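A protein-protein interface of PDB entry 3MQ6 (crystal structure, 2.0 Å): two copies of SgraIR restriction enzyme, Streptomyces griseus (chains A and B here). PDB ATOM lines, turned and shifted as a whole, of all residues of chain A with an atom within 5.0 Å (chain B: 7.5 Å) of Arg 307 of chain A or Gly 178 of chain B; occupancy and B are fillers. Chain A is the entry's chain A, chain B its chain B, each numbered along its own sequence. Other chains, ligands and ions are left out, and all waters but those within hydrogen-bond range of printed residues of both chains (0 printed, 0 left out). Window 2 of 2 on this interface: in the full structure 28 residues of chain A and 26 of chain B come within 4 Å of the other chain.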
ATOM      1  N   GLN A 260     -13.815 -13.045  -1.927  1.00  0.00           N
ATOM      2  CA  GLN A 260     -14.811 -12.736  -2.934  1.00  0.00           C
ATOM      3  C   GLN A 260     -14.889 -13.866  -3.952  1.00  0.00           C
ATOM      4  O   GLN A 260     -15.978 -14.259  -4.366  1.00  0.00           O
ATOM      5  CB  GLN A 260     -14.553 -11.388  -3.582  1.00  0.00           C
ATOM      6  CG  GLN A 260     -15.082 -10.239  -2.720  1.00  0.00           C
ATOM      7  CD  GLN A 260     -14.167  -9.055  -2.701  1.00  0.00           C
ATOM      8  OE1 GLN A 260     -13.332  -8.893  -3.591  1.00  0.00           O
ATOM      9  NE2 GLN A 260     -14.316  -8.203  -1.693  1.00  0.00           N
ATOM     10  N   TYR A 290      -5.987   0.681  -1.950  1.00  0.00           N
ATOM     11  CA  TYR A 290      -7.211  -0.047  -1.654  1.00  0.00           C
ATOM     12  C   TYR A 290      -8.386   0.352  -2.542  1.00  0.00           C
ATOM     13  O   TYR A 290      -9.527   0.000  -2.251  1.00  0.00           O
ATOM     14  CB  TYR A 290      -7.620   0.115  -0.189  1.00  0.00           C
ATOM     15  CG  TYR A 290      -6.722  -0.598   0.801  1.00  0.00           C
ATOM     16  CD1 TYR A 290      -6.335  -1.925   0.607  1.00  0.00           C
ATOM     17  CD2 TYR A 290      -6.277   0.049   1.935  1.00  0.00           C
ATOM     18  CE1 TYR A 290      -5.505  -2.575   1.522  1.00  0.00           C
ATOM     19  CE2 TYR A 290      -5.476  -0.587   2.854  1.00  0.00           C
ATOM     20  CZ  TYR A 290      -5.095  -1.895   2.648  1.00  0.00           C
ATOM     21  OH  TYR A 290      -4.315  -2.497   3.574  1.00  0.00           O
ATOM     22  N   GLU A 291      -8.120   1.079  -3.620  1.00  0.00           N
ATOM     23  CA  GLU A 291      -9.158   1.250  -4.626  1.00  0.00           C
ATOM     24  C   GLU A 291      -9.206   0.065  -5.588  1.00  0.00           C
ATOM     25  O   GLU A 291     -10.075  -0.001  -6.448  1.00  0.00           O
ATOM     26  CB  GLU A 291      -8.951   2.543  -5.394  1.00  0.00           C
ATOM     27  CG  GLU A 291      -9.374   3.751  -4.604  1.00  0.00           C
ATOM     28  CD  GLU A 291      -9.030   5.038  -5.312  1.00  0.00           C
ATOM     29  OE1 GLU A 291      -8.228   4.988  -6.267  1.00  0.00           O
ATOM     30  OE2 GLU A 291      -9.562   6.093  -4.910  1.00  0.00           O
ATOM     31  N   ALA A 292      -8.284  -0.877  -5.428  1.00  0.00           N
ATOM     32  CA  ALA A 292      -8.163  -1.985  -6.375  1.00  0.00           C
ATOM     33  C   ALA A 292      -9.459  -2.773  -6.557  1.00  0.00           C
ATOM     34  O   ALA A 292     -10.073  -3.209  -5.586  1.00  0.00           O
ATOM     35  CB  ALA A 292      -7.022  -2.925  -5.963  1.00  0.00           C
ATOM     36  N   ALA A 293      -9.856  -2.959  -7.815  1.00  0.00           N
ATOM     37  CA  ALA A 293     -11.018  -3.767  -8.148  1.00  0.00           C
ATOM     38  C   ALA A 293     -10.778  -5.206  -7.751  1.00  0.00           C
ATOM     39  O   ALA A 293      -9.656  -5.691  -7.824  1.00  0.00           O
ATOM     40  CB  ALA A 293     -11.297  -3.701  -9.624  1.00  0.00           C
ATOM     41  N   SER A 294     -11.842  -5.885  -7.350  1.00  0.00           N
ATOM     42  CA  SER A 294     -11.779  -7.311  -7.056  1.00  0.00           C
ATOM     43  C   SER A 294     -11.415  -8.076  -8.320  1.00  0.00           C
ATOM     44  O   SER A 294     -12.135  -8.013  -9.317  1.00  0.00           O
ATOM     45  CB  SER A 294     -13.126  -7.783  -6.493  1.00  0.00           C
ATOM     46  OG  SER A 294     -13.402  -9.136  -6.825  1.00  0.00           O
ATOM     47  N   VAL A 305     -18.447  -5.613 -11.251  1.00  0.00           N
ATOM     48  CA  VAL A 305     -17.160  -5.514 -10.574  1.00  0.00           C
ATOM     49  C   VAL A 305     -17.201  -4.459  -9.483  1.00  0.00           C
ATOM     50  O   VAL A 305     -17.760  -3.381  -9.673  1.00  0.00           O
ATOM     51  CB  VAL A 305     -16.038  -5.158 -11.557  1.00  0.00           C
ATOM     52  CG1 VAL A 305     -14.684  -5.450 -10.929  1.00  0.00           C
ATOM     53  CG2 VAL A 305     -16.202  -5.946 -12.843  1.00  0.00           C
ATOM     54  N   HIS A 306     -16.607  -4.778  -8.338  1.00  0.00           N
ATOM     55  CA  HIS A 306     -16.549  -3.847  -7.230  1.00  0.00           C
ATOM     56  C   HIS A 306     -15.176  -3.897  -6.586  1.00  0.00           C
ATOM     57  O   HIS A 306     -14.341  -4.711  -6.957  1.00  0.00           O
ATOM     58  CB  HIS A 306     -17.611  -4.195  -6.195  1.00  0.00           C
ATOM     59  CG  HIS A 306     -17.584  -5.624  -5.769  1.00  0.00           C
ATOM     60  ND1 HIS A 306     -16.575  -6.151  -4.991  1.00  0.00           N
ATOM     61  CD2 HIS A 306     -18.437  -6.646  -6.018  1.00  0.00           C
ATOM     62  CE1 HIS A 306     -16.812  -7.430  -4.773  1.00  0.00           C
ATOM     63  NE2 HIS A 306     -17.936  -7.757  -5.386  1.00  0.00           N
ATOM     64  N   ARG A 307     -14.968  -3.029  -5.604  1.00  0.00           N
ATOM     65  CA  ARG A 307     -13.711  -2.971  -4.883  1.00  0.00           C
ATOM     66  C   ARG A 307     -13.504  -4.197  -3.990  1.00  0.00           C
ATOM     67  O   ARG A 307     -14.445  -4.681  -3.365  1.00  0.00           O
ATOM     68  CB  ARG A 307     -13.661  -1.681  -4.067  1.00  0.00           C
ATOM     69  CG  ARG A 307     -13.490  -0.447  -4.942  1.00  0.00           C
ATOM     70  CD  ARG A 307     -13.685   0.849  -4.179  1.00  0.00           C
ATOM     71  NE  ARG A 307     -12.929   0.831  -2.936  1.00  0.00           N
ATOM     72  CZ  ARG A 307     -12.554   1.918  -2.271  1.00  0.00           C
ATOM     73  NH1 ARG A 307     -12.874   3.110  -2.741  1.00  0.00           N
ATOM     74  NH2 ARG A 307     -11.845   1.808  -1.148  1.00  0.00           N
ATOM     75  N   ALA A 308     -12.273  -4.701  -3.941  1.00  0.00           N
ATOM     76  CA  ALA A 308     -11.914  -5.737  -2.967  1.00  0.00           C
ATOM     77  C   ALA A 308     -12.114  -5.218  -1.538  1.00  0.00           C
ATOM     78  O   ALA A 308     -12.729  -5.881  -0.700  1.00  0.00           O
ATOM     79  CB  ALA A 308     -10.462  -6.178  -3.175  1.00  0.00           C
ATOM     80  N   ILE A 309     -11.586  -4.023  -1.280  1.00  0.00           N
ATOM     81  CA  ILE A 309     -11.667  -3.358   0.019  1.00  0.00           C
ATOM     82  C   ILE A 309     -12.556  -2.134  -0.106  1.00  0.00           C
ATOM     83  O   ILE A 309     -12.258  -1.201  -0.862  1.00  0.00           O
ATOM     84  CB  ILE A 309     -10.269  -2.896   0.500  1.00  0.00           C
ATOM     85  CG1 ILE A 309      -9.311  -4.094   0.620  1.00  0.00           C
ATOM     86  CG2 ILE A 309     -10.349  -2.161   1.825  1.00  0.00           C
ATOM     87  CD1 ILE A 309      -9.669  -5.079   1.727  1.00  0.00           C
ATOM     88  N   ARG A 310     -13.653  -2.139   0.637  1.00  0.00           N
ATOM     89  CA  ARG A 310     -14.676  -1.124   0.478  1.00  0.00           C
ATOM     90  C   ARG A 310     -14.175   0.252   0.918  1.00  0.00           C
ATOM     91  O   ARG A 310     -14.527   1.256   0.319  1.00  0.00           O
ATOM     92  CB  ARG A 310     -15.953  -1.513   1.234  1.00  0.00           C
ATOM     93  CG  ARG A 310     -15.828  -1.455   2.752  1.00  0.00           C
ATOM     94  CD  ARG A 310     -16.910  -2.300   3.422  1.00  0.00           C
ATOM     95  NE  ARG A 310     -18.247  -1.791   3.134  1.00  0.00           N
ATOM     96  CZ  ARG A 310     -18.818  -0.806   3.819  1.00  0.00           C
ATOM     97  NH1 ARG A 310     -18.162  -0.247   4.831  1.00  0.00           N
ATOM     98  NH2 ARG A 310     -20.035  -0.379   3.493  1.00  0.00           N
ATOM     99  N   GLU A 311     -13.349   0.289   1.955  1.00  0.00           N
ATOM    100  CA  GLU A 311     -12.900   1.556   2.517  1.00  0.00           C
ATOM    101  C   GLU A 311     -11.696   1.361   3.416  1.00  0.00           C
ATOM    102  O   GLU A 311     -11.556   0.333   4.080  1.00  0.00           O
ATOM    103  CB  GLU A 311     -14.045   2.239   3.310  1.00  0.00           C
ATOM    104  CG  GLU A 311     -13.665   3.588   3.911  1.00  0.00           C
ATOM    105  CD  GLU A 311     -14.857   4.370   4.499  1.00  0.00           C
ATOM    106  OE1 GLU A 311     -15.977   3.810   4.608  1.00  0.00           O
ATOM    107  OE2 GLU A 311     -14.657   5.558   4.843  1.00  0.00           O
ATOM    108  N   LEU A 312     -10.809   2.347   3.424  1.00  0.00           N
ATOM    109  CA  LEU A 312      -9.801   2.426   4.466  1.00  0.00           C
ATOM    110  C   LEU A 312     -10.280   3.475   5.458  1.00  0.00           C
ATOM    111  O   LEU A 312     -10.307   4.667   5.127  1.00  0.00           O
ATOM    112  CB  LEU A 312      -8.432   2.830   3.885  1.00  0.00           C
ATOM    113  CG  LEU A 312      -7.309   3.113   4.897  1.00  0.00           C
ATOM    114  CD1 LEU A 312      -6.951   1.876   5.761  1.00  0.00           C
ATOM    115  CD2 LEU A 312      -6.081   3.603   4.149  1.00  0.00           C
ATOM    116  N   ALA B 172      -9.029   3.362 -17.309  1.00  0.00           N
ATOM    117  CA  ALA B 172     -10.007   4.418 -17.545  1.00  0.00           C
ATOM    118  C   ALA B 172     -11.411   3.843 -17.473  1.00  0.00           C
ATOM    119  O   ALA B 172     -12.306   4.430 -16.854  1.00  0.00           O
ATOM    120  CB  ALA B 172      -9.766   5.066 -18.903  1.00  0.00           C
ATOM    121  N   GLY B 173     -11.605   2.683 -18.092  1.00  0.00           N
ATOM    122  CA  GLY B 173     -12.876   1.995 -17.989  1.00  0.00           C
ATOM    123  C   GLY B 173     -13.238   1.734 -16.535  1.00  0.00           C
ATOM    124  O   GLY B 173     -14.371   1.969 -16.103  1.00  0.00           O
ATOM    125  N   LEU B 174     -12.264   1.252 -15.772  1.00  0.00           N
ATOM    126  CA  LEU B 174     -12.501   0.927 -14.373  1.00  0.00           C
ATOM    127  C   LEU B 174     -12.895   2.166 -13.585  1.00  0.00           C
ATOM    128  O   LEU B 174     -13.772   2.109 -12.726  1.00  0.00           O
ATOM    129  CB  LEU B 174     -11.262   0.296 -13.747  1.00  0.00           C
ATOM    130  CG  LEU B 174     -10.886  -1.124 -14.162  1.00  0.00           C
ATOM    131  CD1 LEU B 174      -9.644  -1.567 -13.393  1.00  0.00           C
ATOM    132  CD2 LEU B 174     -12.027  -2.103 -13.951  1.00  0.00           C
ATOM    133  N   ARG B 175     -12.231   3.282 -13.876  1.00  0.00           N
ATOM    134  CA  ARG B 175     -12.446   4.514 -13.127  1.00  0.00           C
ATOM    135  C   ARG B 175     -13.859   5.064 -13.282  1.00  0.00           C
ATOM    136  O   ARG B 175     -14.418   5.627 -12.336  1.00  0.00           O
ATOM    137  CB  ARG B 175     -11.415   5.577 -13.507  1.00  0.00           C
ATOM    138  CG  ARG B 175     -10.058   5.351 -12.870  1.00  0.00           C
ATOM    139  CD  ARG B 175      -9.118   6.518 -13.138  1.00  0.00           C
ATOM    140  NE  ARG B 175      -7.744   6.074 -13.389  1.00  0.00           N
ATOM    141  CZ  ARG B 175      -7.169   6.047 -14.590  1.00  0.00           C
ATOM    142  NH1 ARG B 175      -7.844   6.444 -15.665  1.00  0.00           N
ATOM    143  NH2 ARG B 175      -5.914   5.630 -14.717  1.00  0.00           N
ATOM    144  N   LYS B 176     -14.438   4.896 -14.469  1.00  0.00           N
ATOM    145  CA  LYS B 176     -15.797   5.368 -14.702  1.00  0.00           C
ATOM    146  C   LYS B 176     -16.746   4.633 -13.760  1.00  0.00           C
ATOM    147  O   LYS B 176     -17.902   5.018 -13.600  1.00  0.00           O
ATOM    148  CB  LYS B 176     -16.218   5.159 -16.161  1.00  0.00           C
ATOM    149  CG  LYS B 176     -15.355   5.893 -17.188  1.00  0.00           C
ATOM    150  CD  LYS B 176     -15.735   5.493 -18.614  1.00  0.00           C
ATOM    151  CE  LYS B 176     -15.203   6.478 -19.642  1.00  0.00           C
ATOM    152  NZ  LYS B 176     -13.715   6.598 -19.610  1.00  0.00           N
ATOM    153  N   ASP B 177     -16.251   3.573 -13.129  1.00  0.00           N
ATOM    154  CA  ASP B 177     -17.047   2.852 -12.141  1.00  0.00           C
ATOM    155  C   ASP B 177     -16.513   3.051 -10.726  1.00  0.00           C
ATOM    156  O   ASP B 177     -16.907   2.340  -9.811  1.00  0.00           O
ATOM    157  CB  ASP B 177     -17.095   1.359 -12.466  1.00  0.00           C
ATOM    158  CG  ASP B 177     -17.924   1.058 -13.701  1.00  0.00           C
ATOM    159  OD1 ASP B 177     -17.504   0.185 -14.498  1.00  0.00           O
ATOM    160  OD2 ASP B 177     -18.989   1.698 -13.874  1.00  0.00           O
ATOM    161  N   GLY B 178     -15.621   4.020 -10.547  1.00  0.00           N
ATOM    162  CA  GLY B 178     -15.005   4.238  -9.245  1.00  0.00           C
ATOM    163  C   GLY B 178     -14.055   3.133  -8.789  1.00  0.00           C
ATOM    164  O   GLY B 178     -13.921   2.865  -7.588  1.00  0.00           O
ATOM    165  N   LEU B 179     -13.390   2.489  -9.744  1.00  0.00           N
ATOM    166  CA  LEU B 179     -12.414   1.450  -9.430  1.00  0.00           C
ATOM    167  C   LEU B 179     -11.045   1.818  -9.971  1.00  0.00           C
ATOM    168  O   LEU B 179     -10.904   2.742 -10.761  1.00  0.00           O
ATOM    169  CB  LEU B 179     -12.830   0.116 -10.049  1.00  0.00           C
ATOM    170  CG  LEU B 179     -14.225  -0.395  -9.737  1.00  0.00           C
ATOM    171  CD1 LEU B 179     -14.583  -1.577 -10.638  1.00  0.00           C
ATOM    172  CD2 LEU B 179     -14.334  -0.777  -8.267  1.00  0.00           C
ATOM    173  N   GLY B 180     -10.034   1.073  -9.549  1.00  0.00           N
ATOM    174  CA  GLY B 180      -8.705   1.201 -10.120  1.00  0.00           C
ATOM    175  C   GLY B 180      -8.063  -0.169 -10.147  1.00  0.00           C
ATOM    176  O   GLY B 180      -8.662  -1.153  -9.710  1.00  0.00           O
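The backbone carbonyl oxygen of Glu 291 of chain A is in hydrogen-bond range of the backbone NH of Gly 180 of chain B (3.3 Å). O of Gly 180 of chain B lies within hydrogen-bond range of N of Ala 293 of chain A.
O of Tyr 290 of chain A is in hydrogen-bond range of NH2 of Arg 307 of chain A, at 3.1 Å. O of Ala 292 of chain A lies within hydrogen-bond range of N of Ala 308 of chain A (3.1 Å). The backbone NH (N) of Ser 294 of chain A sits at hydrogen-bond distance from the backbone carbonyl oxygen (O) of His 306 of chain A (2.8 Å). NE of Arg 307 of chain A lies within hydrogen-bond range of O of Ile 309 of chain A (3.0 Å). The guanidinium group (NH2) of Arg 307 of chain A lies within hydrogen-bond range of the backbone carbonyl oxygen (O) of Arg 310 of chain A (3.1 Å). O of Leu 174 of chain B is in hydrogen-bond range of N of Leu 179 of chain B (3.0 Å).
No position is printed for both chains. Of the 7 pairs that touch across the chains among the printed residues, none has its exchanged pair printed and touching as well.
Hydrophobic or aromatic side chains of chain B that line the printed part of chain A: Leu 179. Of the 14 printed residues of chain A, 6 touch a printed residue of chain B. Printed residues of chain A that touch a printed residue of chain B: Glu 291, Ala 292, Ala 293, Val 305, His 306 and Arg 307. Among the printed residues, no Asp or Glu carboxylate lies within 4 Å of a Lys or Arg side-chain nitrogen of the other chain.
Ala 292 of chain A touches Gly 180 of chain B. Leu 179 of chain B touches Val 305 of chain A (CD1 to O, 3.8 Å). His 306 of chain A touches Leu 179 of chain B. Gly 178 of chain B touches Arg 307 of chain A. Arg 307 of chain A touches Leu 179 of chain B.
Gly 178 of chain B touches one residue of chain A. Of the printed residues of chain B, Ala 293 of chain A touches Gly 180. Printed residues of chain A within 4 Å of Leu 179 of chain B: Val 305 (3.8 Å), His 306 (3.6 Å) and Arg 307 (3.4 Å). Printed residues of chain B within 4 Å of His 306 of chain A: Leu 179. Of the printed residues of chain B, Glu 291 of chain A touches Gly 180 (3.3 Å). Ala 308 of chain A touches none of the printed residues of chain B. The nearest residue of chain B that does not touch Arg 307 of chain A is Gly 180 of chain B (6.0 Å).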
